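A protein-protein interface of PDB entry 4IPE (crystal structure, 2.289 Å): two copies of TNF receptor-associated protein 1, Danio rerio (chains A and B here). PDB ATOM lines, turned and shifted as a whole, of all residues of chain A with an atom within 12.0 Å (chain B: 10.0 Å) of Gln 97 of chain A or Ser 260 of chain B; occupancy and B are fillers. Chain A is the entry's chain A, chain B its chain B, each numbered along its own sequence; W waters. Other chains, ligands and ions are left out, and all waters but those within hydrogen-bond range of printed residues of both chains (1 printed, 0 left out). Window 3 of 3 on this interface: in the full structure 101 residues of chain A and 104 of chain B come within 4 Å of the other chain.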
ATOM      1  N   ILE A  89     -21.516 -16.449  -8.882  1.00  0.00           N
ATOM      2  CA  ILE A  89     -21.518 -16.625 -10.322  1.00  0.00           C
ATOM      3  C   ILE A  89     -20.105 -16.639 -10.866  1.00  0.00           C
ATOM      4  O   ILE A  89     -19.895 -16.833 -12.064  1.00  0.00           O
ATOM      5  CB  ILE A  89     -22.308 -15.523 -11.025  1.00  0.00           C
ATOM      6  CG1 ILE A  89     -21.618 -14.186 -10.838  1.00  0.00           C
ATOM      7  CG2 ILE A  89     -23.729 -15.457 -10.501  1.00  0.00           C
ATOM      8  CD1 ILE A  89     -22.264 -13.090 -11.625  1.00  0.00           C
ATOM      9  N   THR A  91     -17.078 -18.340 -11.821  1.00  0.00           N
ATOM     10  CA  THR A  91     -16.677 -19.691 -12.180  1.00  0.00           C
ATOM     11  C   THR A  91     -15.616 -19.633 -13.271  1.00  0.00           C
ATOM     12  O   THR A  91     -15.629 -18.726 -14.109  1.00  0.00           O
ATOM     13  CB  THR A  91     -17.870 -20.539 -12.684  1.00  0.00           C
ATOM     14  OG1 THR A  91     -18.608 -19.797 -13.664  1.00  0.00           O
ATOM     15  CG2 THR A  91     -18.799 -20.917 -11.540  1.00  0.00           C
ATOM     16  N   ASP A  92     -14.703 -20.600 -13.257  1.00  0.00           N
ATOM     17  CA  ASP A  92     -13.653 -20.682 -14.267  1.00  0.00           C
ATOM     18  C   ASP A  92     -14.174 -21.309 -15.556  1.00  0.00           C
ATOM     19  O   ASP A  92     -13.978 -22.496 -15.812  1.00  0.00           O
ATOM     20  CB  ASP A  92     -12.455 -21.473 -13.743  1.00  0.00           C
ATOM     21  CG  ASP A  92     -11.277 -21.419 -14.688  1.00  0.00           C
ATOM     22  OD1 ASP A  92     -11.158 -20.407 -15.412  1.00  0.00           O
ATOM     23  OD2 ASP A  92     -10.481 -22.382 -14.716  1.00  0.00           O
ATOM     24  N   THR A  93     -14.840 -20.495 -16.363  1.00  0.00           N
ATOM     25  CA  THR A  93     -15.521 -20.983 -17.553  1.00  0.00           C
ATOM     26  C   THR A  93     -14.850 -20.426 -18.797  1.00  0.00           C
ATOM     27  O   THR A  93     -15.240 -20.752 -19.921  1.00  0.00           O
ATOM     28  CB  THR A  93     -17.008 -20.557 -17.558  1.00  0.00           C
ATOM     29  OG1 THR A  93     -17.099 -19.135 -17.388  1.00  0.00           O
ATOM     30  CG2 THR A  93     -17.765 -21.235 -16.433  1.00  0.00           C
ATOM     31  N   GLU A  94     -13.845 -19.581 -18.583  1.00  0.00           N
ATOM     32  CA  GLU A  94     -13.144 -18.932 -19.685  1.00  0.00           C
ATOM     33  C   GLU A  94     -11.942 -19.729 -20.178  1.00  0.00           C
ATOM     34  O   GLU A  94     -11.244 -20.392 -19.407  1.00  0.00           O
ATOM     35  CB  GLU A  94     -12.693 -17.522 -19.303  1.00  0.00           C
ATOM     36  CG  GLU A  94     -13.817 -16.591 -18.881  1.00  0.00           C
ATOM     37  CD  GLU A  94     -14.136 -16.709 -17.405  1.00  0.00           C
ATOM     38  OE1 GLU A  94     -13.430 -17.465 -16.702  1.00  0.00           O
ATOM     39  OE2 GLU A  94     -15.091 -16.048 -16.949  1.00  0.00           O
ATOM     40  N   ASN A  95     -11.719 -19.655 -21.483  1.00  0.00           N
ATOM     41  CA  ASN A  95     -10.550 -20.254 -22.083  1.00  0.00           C
ATOM     42  C   ASN A  95     -10.002 -19.373 -23.196  1.00  0.00           C
ATOM     43  O   ASN A  95     -10.762 -18.806 -23.984  1.00  0.00           O
ATOM     44  CB  ASN A  95     -10.858 -21.677 -22.551  1.00  0.00           C
ATOM     45  CG  ASN A  95     -10.819 -22.671 -21.406  1.00  0.00           C
ATOM     46  OD1 ASN A  95      -9.870 -22.679 -20.618  1.00  0.00           O
ATOM     47  ND2 ASN A  95     -11.860 -23.488 -21.283  1.00  0.00           N
ATOM     48  N   VAL A  96      -8.681 -19.222 -23.215  1.00  0.00           N
ATOM     49  CA  VAL A  96      -7.993 -18.508 -24.282  1.00  0.00           C
ATOM     50  C   VAL A  96      -8.334 -19.144 -25.630  1.00  0.00           C
ATOM     51  O   VAL A  96      -8.028 -20.315 -25.865  1.00  0.00           O
ATOM     52  CB  VAL A  96      -6.455 -18.563 -24.098  1.00  0.00           C
ATOM     53  CG1 VAL A  96      -5.765 -17.742 -25.174  1.00  0.00           C
ATOM     54  CG2 VAL A  96      -6.045 -18.089 -22.697  1.00  0.00           C
ATOM     55  N   GLN A  97      -8.975 -18.380 -26.508  1.00  0.00           N
ATOM     56  CA  GLN A  97      -9.311 -18.898 -27.834  1.00  0.00           C
ATOM     57  C   GLN A  97      -8.668 -18.064 -28.937  1.00  0.00           C
ATOM     58  O   GLN A  97      -8.905 -16.860 -29.039  1.00  0.00           O
ATOM     59  CB  GLN A  97     -10.827 -18.951 -28.034  1.00  0.00           C
ATOM     60  CG  GLN A  97     -11.597 -19.651 -26.910  1.00  0.00           C
ATOM     61  CD  GLN A  97     -11.520 -21.170 -26.973  1.00  0.00           C
ATOM     62  OE1 GLN A  97     -11.305 -21.750 -28.037  1.00  0.00           O
ATOM     63  NE2 GLN A  97     -11.702 -21.821 -25.827  1.00  0.00           N
ATOM     64  N   GLY A  98      -7.849 -18.718 -29.755  1.00  0.00           N
ATOM     65  CA  GLY A  98      -7.209 -18.066 -30.880  1.00  0.00           C
ATOM     66  C   GLY A  98      -5.970 -17.282 -30.500  1.00  0.00           C
ATOM     67  O   GLY A  98      -5.307 -17.578 -29.502  1.00  0.00           O
ATOM     68  N   SER A  99      -5.664 -16.264 -31.297  1.00  0.00           N
ATOM     69  CA  SER A  99      -4.434 -15.505 -31.127  1.00  0.00           C
ATOM     70  C   SER A  99      -4.667 -14.198 -30.372  1.00  0.00           C
ATOM     71  O   SER A  99      -5.809 -13.847 -30.067  1.00  0.00           O
ATOM     72  CB  SER A  99      -3.784 -15.240 -32.485  1.00  0.00           C
ATOM     73  OG  SER A  99      -2.556 -14.551 -32.330  1.00  0.00           O
ATOM     74  N   PHE A 100      -3.581 -13.488 -30.072  1.00  0.00           N
ATOM     75  CA  PHE A 100      -3.665 -12.267 -29.275  1.00  0.00           C
ATOM     76  C   PHE A 100      -2.781 -11.123 -29.780  1.00  0.00           C
ATOM     77  O   PHE A 100      -1.752 -11.343 -30.417  1.00  0.00           O
ATOM     78  CB  PHE A 100      -3.365 -12.558 -27.800  1.00  0.00           C
ATOM     79  CG  PHE A 100      -1.989 -13.108 -27.556  1.00  0.00           C
ATOM     80  CD1 PHE A 100      -0.910 -12.259 -27.375  1.00  0.00           C
ATOM     81  CD2 PHE A 100      -1.775 -14.476 -27.507  1.00  0.00           C
ATOM     82  CE1 PHE A 100       0.369 -12.765 -27.154  1.00  0.00           C
ATOM     83  CE2 PHE A 100      -0.500 -14.988 -27.283  1.00  0.00           C
ATOM     84  CZ  PHE A 100       0.572 -14.131 -27.105  1.00  0.00           C
ATOM     85  N   SER A 101      -3.202  -9.900 -29.472  1.00  0.00           N
ATOM     86  CA  SER A 101      -2.493  -8.699 -29.879  1.00  0.00           C
ATOM     87  C   SER A 101      -1.676  -8.135 -28.720  1.00  0.00           C
ATOM     88  O   SER A 101      -1.990  -8.371 -27.561  1.00  0.00           O
ATOM     89  CB  SER A 101      -3.496  -7.654 -30.361  1.00  0.00           C
ATOM     90  OG  SER A 101      -4.352  -7.246 -29.315  1.00  0.00           O
ATOM     91  N   VAL B 232      -8.542  -9.549 -17.157  1.00  0.00           N
ATOM     92  CA  VAL B 232      -9.899  -9.055 -17.331  1.00  0.00           C
ATOM     93  C   VAL B 232     -10.645  -9.845 -18.403  1.00  0.00           C
ATOM     94  O   VAL B 232     -10.139 -10.028 -19.513  1.00  0.00           O
ATOM     95  CB  VAL B 232      -9.896  -7.576 -17.709  1.00  0.00           C
ATOM     96  CG1 VAL B 232     -11.305  -7.111 -18.059  1.00  0.00           C
ATOM     97  CG2 VAL B 232      -9.315  -6.754 -16.569  1.00  0.00           C
ATOM     98  N   TYR B 233     -11.843 -10.316 -18.059  1.00  0.00           N
ATOM     99  CA  TYR B 233     -12.713 -11.001 -19.009  1.00  0.00           C
ATOM    100  C   TYR B 233     -13.974 -10.177 -19.167  1.00  0.00           C
ATOM    101  O   TYR B 233     -14.679  -9.922 -18.192  1.00  0.00           O
ATOM    102  CB  TYR B 233     -13.065 -12.403 -18.504  1.00  0.00           C
ATOM    103  CG  TYR B 233     -11.844 -13.274 -18.276  1.00  0.00           C
ATOM    104  CD1 TYR B 233     -11.291 -14.025 -19.308  1.00  0.00           C
ATOM    105  CD2 TYR B 233     -11.240 -13.336 -17.030  1.00  0.00           C
ATOM    106  CE1 TYR B 233     -10.161 -14.815 -19.102  1.00  0.00           C
ATOM    107  CE2 TYR B 233     -10.115 -14.122 -16.817  1.00  0.00           C
ATOM    108  CZ  TYR B 233      -9.574 -14.856 -17.854  1.00  0.00           C
ATOM    109  OH  TYR B 233      -8.447 -15.627 -17.633  1.00  0.00           O
ATOM    110  N   SER B 234     -14.264  -9.754 -20.390  1.00  0.00           N
ATOM    111  CA  SER B 234     -15.436  -8.910 -20.600  1.00  0.00           C
ATOM    112  C   SER B 234     -16.265  -9.314 -21.822  1.00  0.00           C
ATOM    113  O   SER B 234     -15.728  -9.827 -22.806  1.00  0.00           O
ATOM    114  CB  SER B 234     -15.019  -7.439 -20.678  1.00  0.00           C
ATOM    115  OG  SER B 234     -16.150  -6.603 -20.803  1.00  0.00           O
ATOM    116  N   GLN B 235     -17.577  -9.093 -21.736  1.00  0.00           N
ATOM    117  CA  GLN B 235     -18.494  -9.401 -22.835  1.00  0.00           C
ATOM    118  C   GLN B 235     -19.490  -8.261 -23.030  1.00  0.00           C
ATOM    119  O   GLN B 235     -20.293  -7.986 -22.141  1.00  0.00           O
ATOM    120  CB  GLN B 235     -19.240 -10.715 -22.569  1.00  0.00           C
ATOM    121  CG  GLN B 235     -20.409 -10.992 -23.518  1.00  0.00           C
ATOM    122  CD  GLN B 235     -19.969 -11.477 -24.882  1.00  0.00           C
ATOM    123  OE1 GLN B 235     -19.408 -12.563 -25.017  1.00  0.00           O
ATOM    124  NE2 GLN B 235     -20.240 -10.682 -25.907  1.00  0.00           N
ATOM    125  N   ALA B 241     -21.356 -10.407 -30.652  1.00  0.00           N
ATOM    126  CA  ALA B 241     -20.146  -9.715 -30.143  1.00  0.00           C
ATOM    127  C   ALA B 241     -19.330 -10.761 -29.392  1.00  0.00           C
ATOM    128  O   ALA B 241     -19.896 -11.590 -28.678  1.00  0.00           O
ATOM    129  CB  ALA B 241     -20.468  -8.578 -29.194  1.00  0.00           C
ATOM    130  N   PRO B 242     -17.998 -10.723 -29.526  1.00  0.00           N
ATOM    131  CA  PRO B 242     -17.178 -11.786 -28.935  1.00  0.00           C
ATOM    132  C   PRO B 242     -16.797 -11.527 -27.475  1.00  0.00           C
ATOM    133  O   PRO B 242     -17.019 -10.437 -26.947  1.00  0.00           O
ATOM    134  CB  PRO B 242     -15.918 -11.786 -29.816  1.00  0.00           C
ATOM    135  CG  PRO B 242     -16.168 -10.743 -30.917  1.00  0.00           C
ATOM    136  CD  PRO B 242     -17.193  -9.814 -30.353  1.00  0.00           C
ATOM    137  N   GLY B 243     -16.243 -12.553 -26.837  1.00  0.00           N
ATOM    138  CA  GLY B 243     -15.674 -12.424 -25.510  1.00  0.00           C
ATOM    139  C   GLY B 243     -14.200 -12.112 -25.634  1.00  0.00           C
ATOM    140  O   GLY B 243     -13.607 -12.333 -26.693  1.00  0.00           O
ATOM    141  N   TYR B 244     -13.611 -11.585 -24.563  1.00  0.00           N
ATOM    142  CA  TYR B 244     -12.203 -11.200 -24.583  1.00  0.00           C
ATOM    143  C   TYR B 244     -11.502 -11.370 -23.237  1.00  0.00           C
ATOM    144  O   TYR B 244     -12.095 -11.178 -22.173  1.00  0.00           O
ATOM    145  CB  TYR B 244     -12.037  -9.747 -25.032  1.00  0.00           C
ATOM    146  CG  TYR B 244     -12.471  -9.468 -26.452  1.00  0.00           C
ATOM    147  CD1 TYR B 244     -11.627  -9.721 -27.521  1.00  0.00           C
ATOM    148  CD2 TYR B 244     -13.727  -8.939 -26.722  1.00  0.00           C
ATOM    149  CE1 TYR B 244     -12.026  -9.467 -28.824  1.00  0.00           C
ATOM    150  CE2 TYR B 244     -14.133  -8.681 -28.028  1.00  0.00           C
ATOM    151  CZ  TYR B 244     -13.277  -8.947 -29.073  1.00  0.00           C
ATOM    152  OH  TYR B 244     -13.667  -8.696 -30.370  1.00  0.00           O
ATOM    153  N   LYS B 245     -10.223 -11.724 -23.305  1.00  0.00           N
ATOM    154  CA  LYS B 245      -9.381 -11.694 -22.129  1.00  0.00           C
ATOM    155  C   LYS B 245      -8.375 -10.574 -22.286  1.00  0.00           C
ATOM    156  O   LYS B 245      -7.685 -10.496 -23.298  1.00  0.00           O
ATOM    157  CB  LYS B 245      -8.650 -13.012 -21.951  1.00  0.00           C
ATOM    158  CG  LYS B 245      -7.546 -12.938 -20.915  1.00  0.00           C
ATOM    159  CD  LYS B 245      -6.968 -14.313 -20.626  1.00  0.00           C
ATOM    160  CE  LYS B 245      -6.062 -14.275 -19.408  1.00  0.00           C
ATOM    161  NZ  LYS B 245      -5.652 -15.645 -18.984  1.00  0.00           N
ATOM    162  N   VAL B 256      -4.585  -8.750 -25.559  1.00  0.00           N
ATOM    163  CA  VAL B 256      -5.993  -9.122 -25.606  1.00  0.00           C
ATOM    164  C   VAL B 256      -6.222 -10.236 -26.617  1.00  0.00           C
ATOM    165  O   VAL B 256      -5.630 -10.251 -27.700  1.00  0.00           O
ATOM    166  CB  VAL B 256      -6.944  -7.914 -25.878  1.00  0.00           C
ATOM    167  CG1 VAL B 256      -8.399  -8.374 -26.040  1.00  0.00           C
ATOM    168  CG2 VAL B 256      -6.824  -6.848 -24.799  1.00  0.00           C
ATOM    169  N   ALA B 257      -7.060 -11.190 -26.232  1.00  0.00           N
ATOM    170  CA  ALA B 257      -7.426 -12.304 -27.098  1.00  0.00           C
ATOM    171  C   ALA B 257      -8.921 -12.515 -26.990  1.00  0.00           C
ATOM    172  O   ALA B 257      -9.535 -12.142 -25.986  1.00  0.00           O
ATOM    173  CB  ALA B 257      -6.686 -13.568 -26.693  1.00  0.00           C
ATOM    174  N   GLU B 258      -9.508 -13.086 -28.037  1.00  0.00           N
ATOM    175  CA  GLU B 258     -10.911 -13.456 -28.002  1.00  0.00           C
ATOM    176  C   GLU B 258     -11.037 -14.626 -27.046  1.00  0.00           C
ATOM    177  O   GLU B 258     -10.115 -15.435 -26.924  1.00  0.00           O
ATOM    178  CB  GLU B 258     -11.407 -13.831 -29.396  1.00  0.00           C
ATOM    179  CG  GLU B 258     -12.883 -14.192 -29.444  1.00  0.00           C
ATOM    180  CD  GLU B 258     -13.305 -14.697 -30.801  1.00  0.00           C
ATOM    181  OE1 GLU B 258     -12.619 -14.356 -31.788  1.00  0.00           O
ATOM    182  OE2 GLU B 258     -14.313 -15.438 -30.878  1.00  0.00           O
ATOM    183  N   ALA B 259     -12.161 -14.701 -26.344  1.00  0.00           N
ATOM    184  CA  ALA B 259     -12.364 -15.771 -25.380  1.00  0.00           C
ATOM    185  C   ALA B 259     -13.798 -16.304 -25.396  1.00  0.00           C
ATOM    186  O   ALA B 259     -14.723 -15.625 -25.848  1.00  0.00           O
ATOM    187  CB  ALA B 259     -11.972 -15.297 -23.984  1.00  0.00           C
ATOM    188  N   SER B 260     -13.964 -17.535 -24.919  1.00  0.00           N
ATOM    189  CA  SER B 260     -15.278 -18.149 -24.780  1.00  0.00           C
ATOM    190  C   SER B 260     -15.558 -18.391 -23.302  1.00  0.00           C
ATOM    191  O   SER B 260     -14.636 -18.373 -22.482  1.00  0.00           O
ATOM    192  CB  SER B 260     -15.332 -19.478 -25.532  1.00  0.00           C
ATOM    193  OG  SER B 260     -14.477 -20.437 -24.929  1.00  0.00           O
ATOM    194  N   GLY B 261     -16.825 -18.635 -22.967  1.00  0.00           N
ATOM    195  CA  GLY B 261     -17.233 -18.786 -21.580  1.00  0.00           C
ATOM    196  C   GLY B 261     -17.189 -17.468 -20.829  1.00  0.00           C
ATOM    197  O   GLY B 261     -17.058 -17.440 -19.595  1.00  0.00           O
ATOM    198  N   VAL B 262     -17.278 -16.363 -21.563  1.00  0.00           N
ATOM    199  CA  VAL B 262     -17.322 -15.065 -20.903  1.00  0.00           C
ATOM    200  C   VAL B 262     -18.764 -14.623 -20.725  1.00  0.00           C
ATOM    201  O   VAL B 262     -19.474 -14.356 -21.698  1.00  0.00           O
ATOM    202  CB  VAL B 262     -16.517 -13.972 -21.631  1.00  0.00           C
ATOM    203  CG1 VAL B 262     -16.706 -12.643 -20.918  1.00  0.00           C
ATOM    204  CG2 VAL B 262     -15.025 -14.345 -21.693  1.00  0.00           C
ATOM    205  N   ARG B 263     -19.185 -14.572 -19.464  1.00  0.00           N
ATOM    206  CA  ARG B 263     -20.523 -14.130 -19.111  1.00  0.00           C
ATOM    207  C   ARG B 263     -20.665 -12.629 -19.349  1.00  0.00           C
ATOM    208  O   ARG B 263     -19.703 -11.868 -19.198  1.00  0.00           O
ATOM    209  CB  ARG B 263     -20.830 -14.484 -17.650  1.00  0.00           C
ATOM    210  CG  ARG B 263     -22.190 -14.018 -17.146  1.00  0.00           C
ATOM    211  CD  ARG B 263     -22.539 -14.715 -15.847  1.00  0.00           C
ATOM    212  NE  ARG B 263     -23.594 -14.031 -15.108  1.00  0.00           N
ATOM    213  CZ  ARG B 263     -24.897 -14.234 -15.296  1.00  0.00           C
ATOM    214  NH1 ARG B 263     -25.322 -15.094 -16.219  1.00  0.00           N
ATOM    215  NH2 ARG B 263     -25.781 -13.564 -14.563  1.00  0.00           N
ATOM    216  N   GLN B 264     -21.862 -12.232 -19.768  1.00  0.00           N
ATOM    217  CA  GLN B 264     -22.222 -10.833 -19.896  1.00  0.00           C
ATOM    218  C   GLN B 264     -21.721 -10.044 -18.693  1.00  0.00           C
ATOM    219  O   GLN B 264     -22.055 -10.361 -17.551  1.00  0.00           O
ATOM    220  CB  GLN B 264     -23.740 -10.706 -20.009  1.00  0.00           C
ATOM    221  CG  GLN B 264     -24.250  -9.275 -19.931  1.00  0.00           C
ATOM    222  CD  GLN B 264     -23.938  -8.478 -21.175  1.00  0.00           C
ATOM    223  OE1 GLN B 264     -24.069  -8.978 -22.294  1.00  0.00           O
ATOM    224  NE2 GLN B 264     -23.521  -7.231 -20.990  1.00  0.00           N
ATOM    225  N   LYS B 267     -15.336  -9.697 -15.513  1.00  0.00           N
ATOM    226  CA  LYS B 267     -14.666 -10.298 -14.370  1.00  0.00           C
ATOM    227  C   LYS B 267     -13.219  -9.873 -14.370  1.00  0.00           C
ATOM    228  O   LYS B 267     -12.555  -9.884 -15.414  1.00  0.00           O
ATOM    229  CB  LYS B 267     -14.745 -11.826 -14.423  1.00  0.00           C
ATOM    230  CG  LYS B 267     -14.035 -12.508 -13.269  1.00  0.00           C
ATOM    231  CD  LYS B 267     -14.357 -13.996 -13.228  1.00  0.00           C
ATOM    232  CE  LYS B 267     -13.765 -14.723 -14.406  1.00  0.00           C
ATOM    233  NZ  LYS B 267     -14.000 -16.199 -14.288  1.00  0.00           N
HETATM  234  O   HOH W   1     -17.006 -16.352 -13.494  1.00  0.00           O
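Water W1 lies within hydrogen-bond range of the backbone NH of Thr 91 of chain A, the side-chain amino group of Lys 267 of chain B and the backbone carbonyl oxygen of Ile 89 of chain A.
Gln 97 of chain A touches two residues of chain B.
Ser 260 of chain B touches four residues of chain A.
No residue of chain B comes within 4 Å of Val 96 of chain A.
Of chain A, only Gln 97 comes within 4 Å of Glu 258 of chain B.
Ala 259 of chain B touches one residue of chain A.
Of the printed residues of chain A, Val 256 of chain B touches Phe 100 and Ser 101.
Of the printed residues of chain B, Ser 99 of chain A touches Ala 257 (3.5 Å).
Of the printed residues of chain B, Ser 101 of chain A touches Val 256.
Lys 245 of chain B touches none of the printed residues of chain A.
Pro 242 of chain B touches none of the printed residues of chain A.
The nearest residue of chain A that does not touch Ser 260 of chain B is Val 96 of chain A (5.8 Å).
The nearest printed residue of chain B that does not touch Ser 101 of chain A is Ala 257 of chain B (5.2 Å).
Of the 19 printed residues of chain B, 10 touch a printed residue of chain A.
Printed residues of chain B that touch a printed residue of chain A: Tyr 233, Val 256, Ala 257, Glu 258, Ala 259, Ser 260, Gly 261, Val 262, Arg 263 and Lys 267.
Hydrophobic or aromatic side chains of chain A that line the printed part of chain B: Ile 89 and Phe 100.
Among the printed residues, Asp or Glu carboxylates within 4 Å of a Lys or Arg side-chain nitrogen of the other chain: Glu 94 of chain A with Lys 267 of chain B (2.8 Å).
No position is printed for both chains.
Among the printed residues, pairs that only touch across the chains: Glu 94 of chain A with Ser 260 of chain B (3.2 Å), Phe 100 of chain A with Val 256 of chain B (3.2 Å), Glu 94 of chain A with Gly 261 of chain B (3.4 Å), Ser 99 of chain A with Ala 257 of chain B (3.5 Å), Thr 93 of chain A with Ser 260 of chain B (3.5 Å), Glu 94 of chain A with Tyr 233 of chain B (3.6 Å), Phe 100 of chain A with Ala 257 of chain B (3.6 Å), Asn 95 of chain A with Ala 259 of chain B (3.7 Å), Glu 94 of chain A with Val 262 of chain B (3.8 Å) and Ile 89 of chain A with Arg 263 of chain B (3.8 Å).
The side-chain hydroxyl (OH) of Tyr 233 of chain B lies within hydrogen-bond range of the side-chain amino group (NZ) of Lys 245 of chain B, 3.1 Å away.
The backbone carbonyl oxygen of Tyr 233 of chain B lies within hydrogen-bond range of the backbone NH of Lys 267 of chain B (2.8 Å).
O of Gly 243 of chain B sits at hydrogen-bond distance from N of Ala 259 of chain B (2.8 Å).
O of Ala 257 of chain B is in hydrogen-bond range of N of Lys 245 of chain B (2.8 Å).
The backbone carbonyl oxygen (O) of Thr 91 of chain A lies within hydrogen-bond range of the side-chain amino group (NZ) of Lys 267 of chain B, 3.0 Å away.
The side-chain hydroxyl (OG1) of Thr 93 of chain A sits at hydrogen-bond distance from the backbone carbonyl oxygen (O) of Gly 261 of chain B, at 2.8 Å.
OE1 of Glu 94 of chain A lies within salt-bridge range of NZ of Lys 267 of chain B.
N of Asn 95 of chain A lies within hydrogen-bond range of O of Ser 260 of chain B, at 3.3 Å.
O of Glu 258 of chain B sits at hydrogen-bond distance from N of Gln 97 of chain A (3.2 Å).
NE2 of Gln 97 of chain A sits at hydrogen-bond distance from OG of Ser 260 of chain B (3.2 Å).
The backbone NH (N) of Ser 101 of chain A is in hydrogen-bond range of the backbone carbonyl oxygen (O) of Val 256 of chain B (3.0 Å).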
